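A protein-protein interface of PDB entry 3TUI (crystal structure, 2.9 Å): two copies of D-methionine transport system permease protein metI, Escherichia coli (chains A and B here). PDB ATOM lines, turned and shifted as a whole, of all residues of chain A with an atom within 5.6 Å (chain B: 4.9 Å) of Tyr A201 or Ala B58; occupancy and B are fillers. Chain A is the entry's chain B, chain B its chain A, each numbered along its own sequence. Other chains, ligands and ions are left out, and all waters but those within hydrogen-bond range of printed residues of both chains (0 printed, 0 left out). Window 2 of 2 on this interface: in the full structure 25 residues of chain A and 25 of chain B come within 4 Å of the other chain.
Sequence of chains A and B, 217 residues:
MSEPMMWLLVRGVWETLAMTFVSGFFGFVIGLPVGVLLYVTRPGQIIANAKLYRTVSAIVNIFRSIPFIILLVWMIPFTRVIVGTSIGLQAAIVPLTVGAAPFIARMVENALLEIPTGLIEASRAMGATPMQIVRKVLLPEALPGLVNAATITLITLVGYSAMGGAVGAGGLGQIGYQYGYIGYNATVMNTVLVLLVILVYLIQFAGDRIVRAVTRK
Among the printed residues, merely in contact across the chains: Val A197 with Ser B65 (3.9 Å), Val A200 with Ser B65 (3.1 Å), Tyr A201 with Ala B58 (3.9 Å), Tyr A201 with Asn B61 (3.8 Å), Tyr A201 with Ile B62 (3.7 Å) and Tyr A201 with Ser B65 (3.9 Å).
No position is printed for both chains. Of the 6 pairs that touch across the chains among the printed residues, none has its exchanged pair printed and touching as well.
Of the 11 printed residues of chain B, 4 touch a printed residue of chain A. Hydrophobic or aromatic side chains of chain B that line the printed part of chain A: Ile B62. Along chain A the printed residues that touch a printed residue of chain B span positions 197 to 201.
Printed residues of chain B within 4 Å of Val A200: Ser B65 (3.1 Å). Of chain B, only Ala B58, Asn B61, Ile B62 and Ser B65 come within 4 Å of Tyr A201. Tyr B53 touches none of the printed residues of chain A. Val B56 touches none of the printed residues of chain A. Ala B58 touches just one residue of chain A: Tyr A201 (3.9 Å). Of the printed residues of chain A, Ile B62 touches Tyr A201 (3.7 Å). Of the printed residues of chain A, Ser B65 touches Val A197 (3.9 Å), Val A200 (3.1 Å) and Tyr A201 (3.9 Å). The nearest printed residue of chain B that does not touch Tyr A201 is Ile B59 (6.1 Å). The nearest printed residue of chain A that does not touch Ala B58 is Val A197 (7.8 Å). The nearest printed residue of chain A that does not touch Ile B62 is Val A197 (4.8 Å).
ND2 of Asn B61 sits at hydrogen-bond distance from O of Ser B57, 2.6 Å away.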
ATOM      1  N   LEU A 196      -7.663  17.803   6.085  1.00  0.00           N
ATOM      2  CA  LEU A 196      -7.238  16.794   7.047  1.00  0.00           C
ATOM      3  C   LEU A 196      -5.712  16.776   7.279  1.00  0.00           C
ATOM      4  O   LEU A 196      -5.242  16.685   8.429  1.00  0.00           O
ATOM      5  CB  LEU A 196      -7.750  15.418   6.631  1.00  0.00           C
ATOM      6  CG  LEU A 196      -9.255  15.204   6.791  1.00  0.00           C
ATOM      7  CD1 LEU A 196      -9.581  13.911   6.071  1.00  0.00           C
ATOM      8  CD2 LEU A 196      -9.704  15.134   8.262  1.00  0.00           C
ATOM      9  N   VAL A 197      -4.951  16.859   6.186  1.00  0.00           N
ATOM     10  CA  VAL A 197      -3.507  16.974   6.280  1.00  0.00           C
ATOM     11  C   VAL A 197      -3.195  18.122   7.221  1.00  0.00           C
ATOM     12  O   VAL A 197      -2.409  17.969   8.158  1.00  0.00           O
ATOM     13  CB  VAL A 197      -2.842  17.187   4.903  1.00  0.00           C
ATOM     14  CG1 VAL A 197      -1.345  17.319   5.056  1.00  0.00           C
ATOM     15  CG2 VAL A 197      -3.159  16.032   3.980  1.00  0.00           C
ATOM     16  N   ILE A 198      -3.842  19.259   6.985  1.00  0.00           N
ATOM     17  CA  ILE A 198      -3.732  20.413   7.874  1.00  0.00           C
ATOM     18  C   ILE A 198      -4.047  20.077   9.335  1.00  0.00           C
ATOM     19  O   ILE A 198      -3.419  20.611  10.246  1.00  0.00           O
ATOM     20  CB  ILE A 198      -4.638  21.576   7.401  1.00  0.00           C
ATOM     21  CG1 ILE A 198      -4.068  22.197   6.119  1.00  0.00           C
ATOM     22  CG2 ILE A 198      -4.783  22.624   8.486  1.00  0.00           C
ATOM     23  CD1 ILE A 198      -2.660  22.759   6.284  1.00  0.00           C
ATOM     24  N   LEU A 199      -5.005  19.181   9.551  1.00  0.00           N
ATOM     25  CA  LEU A 199      -5.444  18.830  10.899  1.00  0.00           C
ATOM     26  C   LEU A 199      -4.472  17.914  11.648  1.00  0.00           C
ATOM     27  O   LEU A 199      -4.341  17.980  12.884  1.00  0.00           O
ATOM     28  CB  LEU A 199      -6.821  18.186  10.870  1.00  0.00           C
ATOM     29  CG  LEU A 199      -7.357  17.950  12.282  1.00  0.00           C
ATOM     30  CD1 LEU A 199      -7.566  19.285  12.992  1.00  0.00           C
ATOM     31  CD2 LEU A 199      -8.671  17.217  12.219  1.00  0.00           C
ATOM     32  N   VAL A 200      -3.818  17.024  10.904  1.00  0.00           N
ATOM     33  CA  VAL A 200      -2.774  16.195  11.497  1.00  0.00           C
ATOM     34  C   VAL A 200      -1.623  17.066  12.006  1.00  0.00           C
ATOM     35  O   VAL A 200      -1.218  16.940  13.162  1.00  0.00           O
ATOM     36  CB  VAL A 200      -2.252  15.125  10.515  1.00  0.00           C
ATOM     37  CG1 VAL A 200      -0.944  14.503  11.034  1.00  0.00           C
ATOM     38  CG2 VAL A 200      -3.333  14.066  10.254  1.00  0.00           C
ATOM     39  N   TYR A 201      -1.126  17.961  11.146  1.00  0.00           N
ATOM     40  CA  TYR A 201      -0.011  18.856  11.483  1.00  0.00           C
ATOM     41  C   TYR A 201      -0.308  19.725  12.703  1.00  0.00           C
ATOM     42  O   TYR A 201       0.509  19.850  13.605  1.00  0.00           O
ATOM     43  CB  TYR A 201       0.357  19.736  10.290  1.00  0.00           C
ATOM     44  CG  TYR A 201       1.275  19.066   9.290  1.00  0.00           C
ATOM     45  CD1 TYR A 201       1.055  17.755   8.888  1.00  0.00           C
ATOM     46  CD2 TYR A 201       2.347  19.752   8.729  1.00  0.00           C
ATOM     47  CE1 TYR A 201       1.885  17.139   7.970  1.00  0.00           C
ATOM     48  CE2 TYR A 201       3.181  19.143   7.806  1.00  0.00           C
ATOM     49  CZ  TYR A 201       2.945  17.835   7.434  1.00  0.00           C
ATOM     50  OH  TYR A 201       3.763  17.212   6.520  1.00  0.00           O
ATOM     51  N   LEU A 202      -1.487  20.325  12.730  1.00  0.00           N
ATOM     52  CA  LEU A 202      -1.883  21.123  13.885  1.00  0.00           C
ATOM     53  C   LEU A 202      -1.911  20.292  15.167  1.00  0.00           C
ATOM     54  O   LEU A 202      -1.433  20.749  16.208  1.00  0.00           O
ATOM     55  CB  LEU A 202      -3.225  21.824  13.637  1.00  0.00           C
ATOM     56  CG  LEU A 202      -3.073  23.314  13.310  1.00  0.00           C
ATOM     57  CD1 LEU A 202      -2.218  23.550  12.075  1.00  0.00           C
ATOM     58  CD2 LEU A 202      -4.434  23.961  13.172  1.00  0.00           C
ATOM     59  N   ILE A 203      -2.451  19.075  15.095  1.00  0.00           N
ATOM     60  CA  ILE A 203      -2.413  18.180  16.251  1.00  0.00           C
ATOM     61  C   ILE A 203      -0.985  17.876  16.680  1.00  0.00           C
ATOM     62  O   ILE A 203      -0.690  17.820  17.873  1.00  0.00           O
ATOM     63  CB  ILE A 203      -3.173  16.858  16.012  1.00  0.00           C
ATOM     64  CG1 ILE A 203      -4.663  17.139  15.806  1.00  0.00           C
ATOM     65  CG2 ILE A 203      -3.012  15.930  17.210  1.00  0.00           C
ATOM     66  CD1 ILE A 203      -5.222  18.191  16.790  1.00  0.00           C
ATOM     67  N   GLN A 204      -0.093  17.669  15.714  1.00  0.00           N
ATOM     68  CA  GLN A 204       1.265  17.338  16.095  1.00  0.00           C
ATOM     69  C   GLN A 204       2.096  18.546  16.456  1.00  0.00           C
ATOM     70  O   GLN A 204       2.854  18.495  17.402  1.00  0.00           O
ATOM     71  CB  GLN A 204       1.974  16.461  15.083  1.00  0.00           C
ATOM     72  CG  GLN A 204       3.061  15.673  15.766  1.00  0.00           C
ATOM     73  CD  GLN A 204       3.784  14.742  14.835  1.00  0.00           C
ATOM     74  OE1 GLN A 204       3.232  14.323  13.812  1.00  0.00           O
ATOM     75  NE2 GLN A 204       5.026  14.387  15.189  1.00  0.00           N
ATOM     76  N   PHE A 205       1.956  19.644  15.731  1.00  0.00           N
ATOM     77  CA  PHE A 205       2.713  20.827  16.105  1.00  0.00           C
ATOM     78  C   PHE A 205       2.343  21.249  17.520  1.00  0.00           C
ATOM     79  O   PHE A 205       3.222  21.570  18.312  1.00  0.00           O
ATOM     80  CB  PHE A 205       2.532  21.952  15.084  1.00  0.00           C
ATOM     81  CG  PHE A 205       3.391  21.786  13.848  1.00  0.00           C
ATOM     82  CD1 PHE A 205       4.690  21.297  13.955  1.00  0.00           C
ATOM     83  CD2 PHE A 205       2.900  22.102  12.578  1.00  0.00           C
ATOM     84  CE1 PHE A 205       5.496  21.131  12.823  1.00  0.00           C
ATOM     85  CE2 PHE A 205       3.699  21.936  11.439  1.00  0.00           C
ATOM     86  CZ  PHE A 205       4.997  21.453  11.564  1.00  0.00           C
ATOM     87  N   ALA A 206       1.057  21.199  17.854  1.00  0.00           N
ATOM     88  CA  ALA A 206       0.608  21.443  19.233  1.00  0.00           C
ATOM     89  C   ALA A 206       1.282  20.542  20.274  1.00  0.00           C
ATOM     90  O   ALA A 206       1.828  21.038  21.264  1.00  0.00           O
ATOM     91  CB  ALA A 206      -0.901  21.284  19.349  1.00  0.00           C
ATOM     92  N   TYR B  53      17.326  15.896   1.963  1.00  0.00           N
ATOM     93  CA  TYR B  53      16.645  15.221   3.055  1.00  0.00           C
ATOM     94  C   TYR B  53      15.309  15.922   3.318  1.00  0.00           C
ATOM     95  O   TYR B  53      14.258  15.296   3.204  1.00  0.00           O
ATOM     96  CB  TYR B  53      17.515  15.174   4.329  1.00  0.00           C
ATOM     97  CG  TYR B  53      16.874  14.392   5.455  1.00  0.00           C
ATOM     98  CD1 TYR B  53      16.945  13.002   5.496  1.00  0.00           C
ATOM     99  CD2 TYR B  53      16.164  15.036   6.459  1.00  0.00           C
ATOM    100  CE1 TYR B  53      16.333  12.275   6.524  1.00  0.00           C
ATOM    101  CE2 TYR B  53      15.553  14.322   7.490  1.00  0.00           C
ATOM    102  CZ  TYR B  53      15.640  12.944   7.518  1.00  0.00           C
ATOM    103  OH  TYR B  53      15.034  12.235   8.537  1.00  0.00           O
ATOM    104  N   ARG B  54      15.349  17.222   3.611  1.00  0.00           N
ATOM    105  CA  ARG B  54      14.146  17.991   3.961  1.00  0.00           C
ATOM    106  C   ARG B  54      12.973  17.759   3.015  1.00  0.00           C
ATOM    107  O   ARG B  54      11.828  17.623   3.451  1.00  0.00           O
ATOM    108  CB  ARG B  54      14.462  19.489   4.006  1.00  0.00           C
ATOM    109  CG  ARG B  54      15.317  19.938   5.185  1.00  0.00           C
ATOM    110  CD  ARG B  54      14.452  20.133   6.419  1.00  0.00           C
ATOM    111  NE  ARG B  54      13.241  20.892   6.102  1.00  0.00           N
ATOM    112  CZ  ARG B  54      13.193  22.216   5.969  1.00  0.00           C
ATOM    113  NH1 ARG B  54      14.288  22.948   6.148  1.00  0.00           N
ATOM    114  NH2 ARG B  54      12.041  22.811   5.672  1.00  0.00           N
ATOM    115  N   THR B  55      13.270  17.729   1.720  1.00  0.00           N
ATOM    116  CA  THR B  55      12.260  17.513   0.686  1.00  0.00           C
ATOM    117  C   THR B  55      11.644  16.108   0.772  1.00  0.00           C
ATOM    118  O   THR B  55      10.423  15.955   0.907  1.00  0.00           O
ATOM    119  CB  THR B  55      12.853  17.778  -0.732  1.00  0.00           C
ATOM    120  OG1 THR B  55      12.950  19.192  -0.958  1.00  0.00           O
ATOM    121  CG2 THR B  55      11.987  17.157  -1.826  1.00  0.00           C
ATOM    122  N   VAL B  56      12.495  15.088   0.712  1.00  0.00           N
ATOM    123  CA  VAL B  56      12.030  13.714   0.806  1.00  0.00           C
ATOM    124  C   VAL B  56      11.331  13.465   2.154  1.00  0.00           C
ATOM    125  O   VAL B  56      10.364  12.709   2.229  1.00  0.00           O
ATOM    126  CB  VAL B  56      13.188  12.708   0.592  1.00  0.00           C
ATOM    127  CG1 VAL B  56      12.668  11.278   0.564  1.00  0.00           C
ATOM    128  CG2 VAL B  56      13.919  13.011  -0.708  1.00  0.00           C
ATOM    129  N   SER B  57      11.797  14.119   3.215  1.00  0.00           N
ATOM    130  CA  SER B  57      11.241  13.880   4.554  1.00  0.00           C
ATOM    131  C   SER B  57       9.855  14.529   4.746  1.00  0.00           C
ATOM    132  O   SER B  57       8.992  13.979   5.442  1.00  0.00           O
ATOM    133  CB  SER B  57      12.223  14.340   5.651  1.00  0.00           C
ATOM    134  OG  SER B  57      11.787  13.964   6.951  1.00  0.00           O
ATOM    135  N   ALA B  58       9.642  15.688   4.127  1.00  0.00           N
ATOM    136  CA  ALA B  58       8.362  16.384   4.218  1.00  0.00           C
ATOM    137  C   ALA B  58       7.271  15.653   3.441  1.00  0.00           C
ATOM    138  O   ALA B  58       6.122  15.562   3.896  1.00  0.00           O
ATOM    139  CB  ALA B  58       8.503  17.812   3.730  1.00  0.00           C
ATOM    140  N   ILE B  59       7.648  15.136   2.269  1.00  0.00           N
ATOM    141  CA  ILE B  59       6.689  14.505   1.361  1.00  0.00           C
ATOM    142  C   ILE B  59       6.224  13.162   1.930  1.00  0.00           C
ATOM    143  O   ILE B  59       5.029  12.842   1.886  1.00  0.00           O
ATOM    144  CB  ILE B  59       7.229  14.369  -0.115  1.00  0.00           C
ATOM    145  CG1 ILE B  59       8.364  13.346  -0.248  1.00  0.00           C
ATOM    146  CG2 ILE B  59       7.616  15.736  -0.688  1.00  0.00           C
ATOM    147  CD1 ILE B  59       8.537  12.813  -1.663  1.00  0.00           C
ATOM    148  N   VAL B  60       7.165  12.389   2.478  1.00  0.00           N
ATOM    149  CA  VAL B  60       6.795  11.148   3.147  1.00  0.00           C
ATOM    150  C   VAL B  60       5.852  11.488   4.296  1.00  0.00           C
ATOM    151  O   VAL B  60       4.896  10.762   4.559  1.00  0.00           O
ATOM    152  CB  VAL B  60       8.019  10.297   3.662  1.00  0.00           C
ATOM    153  CG1 VAL B  60       8.902   9.840   2.514  1.00  0.00           C
ATOM    154  CG2 VAL B  60       8.822  11.049   4.689  1.00  0.00           C
ATOM    155  N   ASN B  61       6.116  12.607   4.961  1.00  0.00           N
ATOM    156  CA  ASN B  61       5.281  13.037   6.072  1.00  0.00           C
ATOM    157  C   ASN B  61       3.906  13.440   5.587  1.00  0.00           C
ATOM    158  O   ASN B  61       2.893  13.125   6.218  1.00  0.00           O
ATOM    159  CB  ASN B  61       5.948  14.180   6.837  1.00  0.00           C
ATOM    160  CG  ASN B  61       6.990  13.688   7.826  1.00  0.00           C
ATOM    161  OD1 ASN B  61       6.760  12.730   8.567  1.00  0.00           O
ATOM    162  ND2 ASN B  61       8.143  14.350   7.845  1.00  0.00           N
ATOM    163  N   ILE B  62       3.883  14.143   4.459  1.00  0.00           N
ATOM    164  CA  ILE B  62       2.637  14.480   3.778  1.00  0.00           C
ATOM    165  C   ILE B  62       1.867  13.223   3.402  1.00  0.00           C
ATOM    166  O   ILE B  62       0.714  13.050   3.804  1.00  0.00           O
ATOM    167  CB  ILE B  62       2.900  15.337   2.522  1.00  0.00           C
ATOM    168  CG1 ILE B  62       2.967  16.821   2.903  1.00  0.00           C
ATOM    169  CG2 ILE B  62       1.828  15.098   1.470  1.00  0.00           C
ATOM    170  CD1 ILE B  62       3.667  17.698   1.879  1.00  0.00           C
ATOM    171  N   SER B  65       0.591  11.368   6.290  1.00  0.00           N
ATOM    172  CA  SER B  65      -0.382  12.103   7.082  1.00  0.00           C
ATOM    173  C   SER B  65      -1.805  12.097   6.478  1.00  0.00           C
ATOM    174  O   SER B  65      -2.737  12.648   7.064  1.00  0.00           O
ATOM    175  CB  SER B  65       0.121  13.530   7.312  1.00  0.00           C
ATOM    176  OG  SER B  65      -0.886  14.347   7.870  1.00  0.00           O
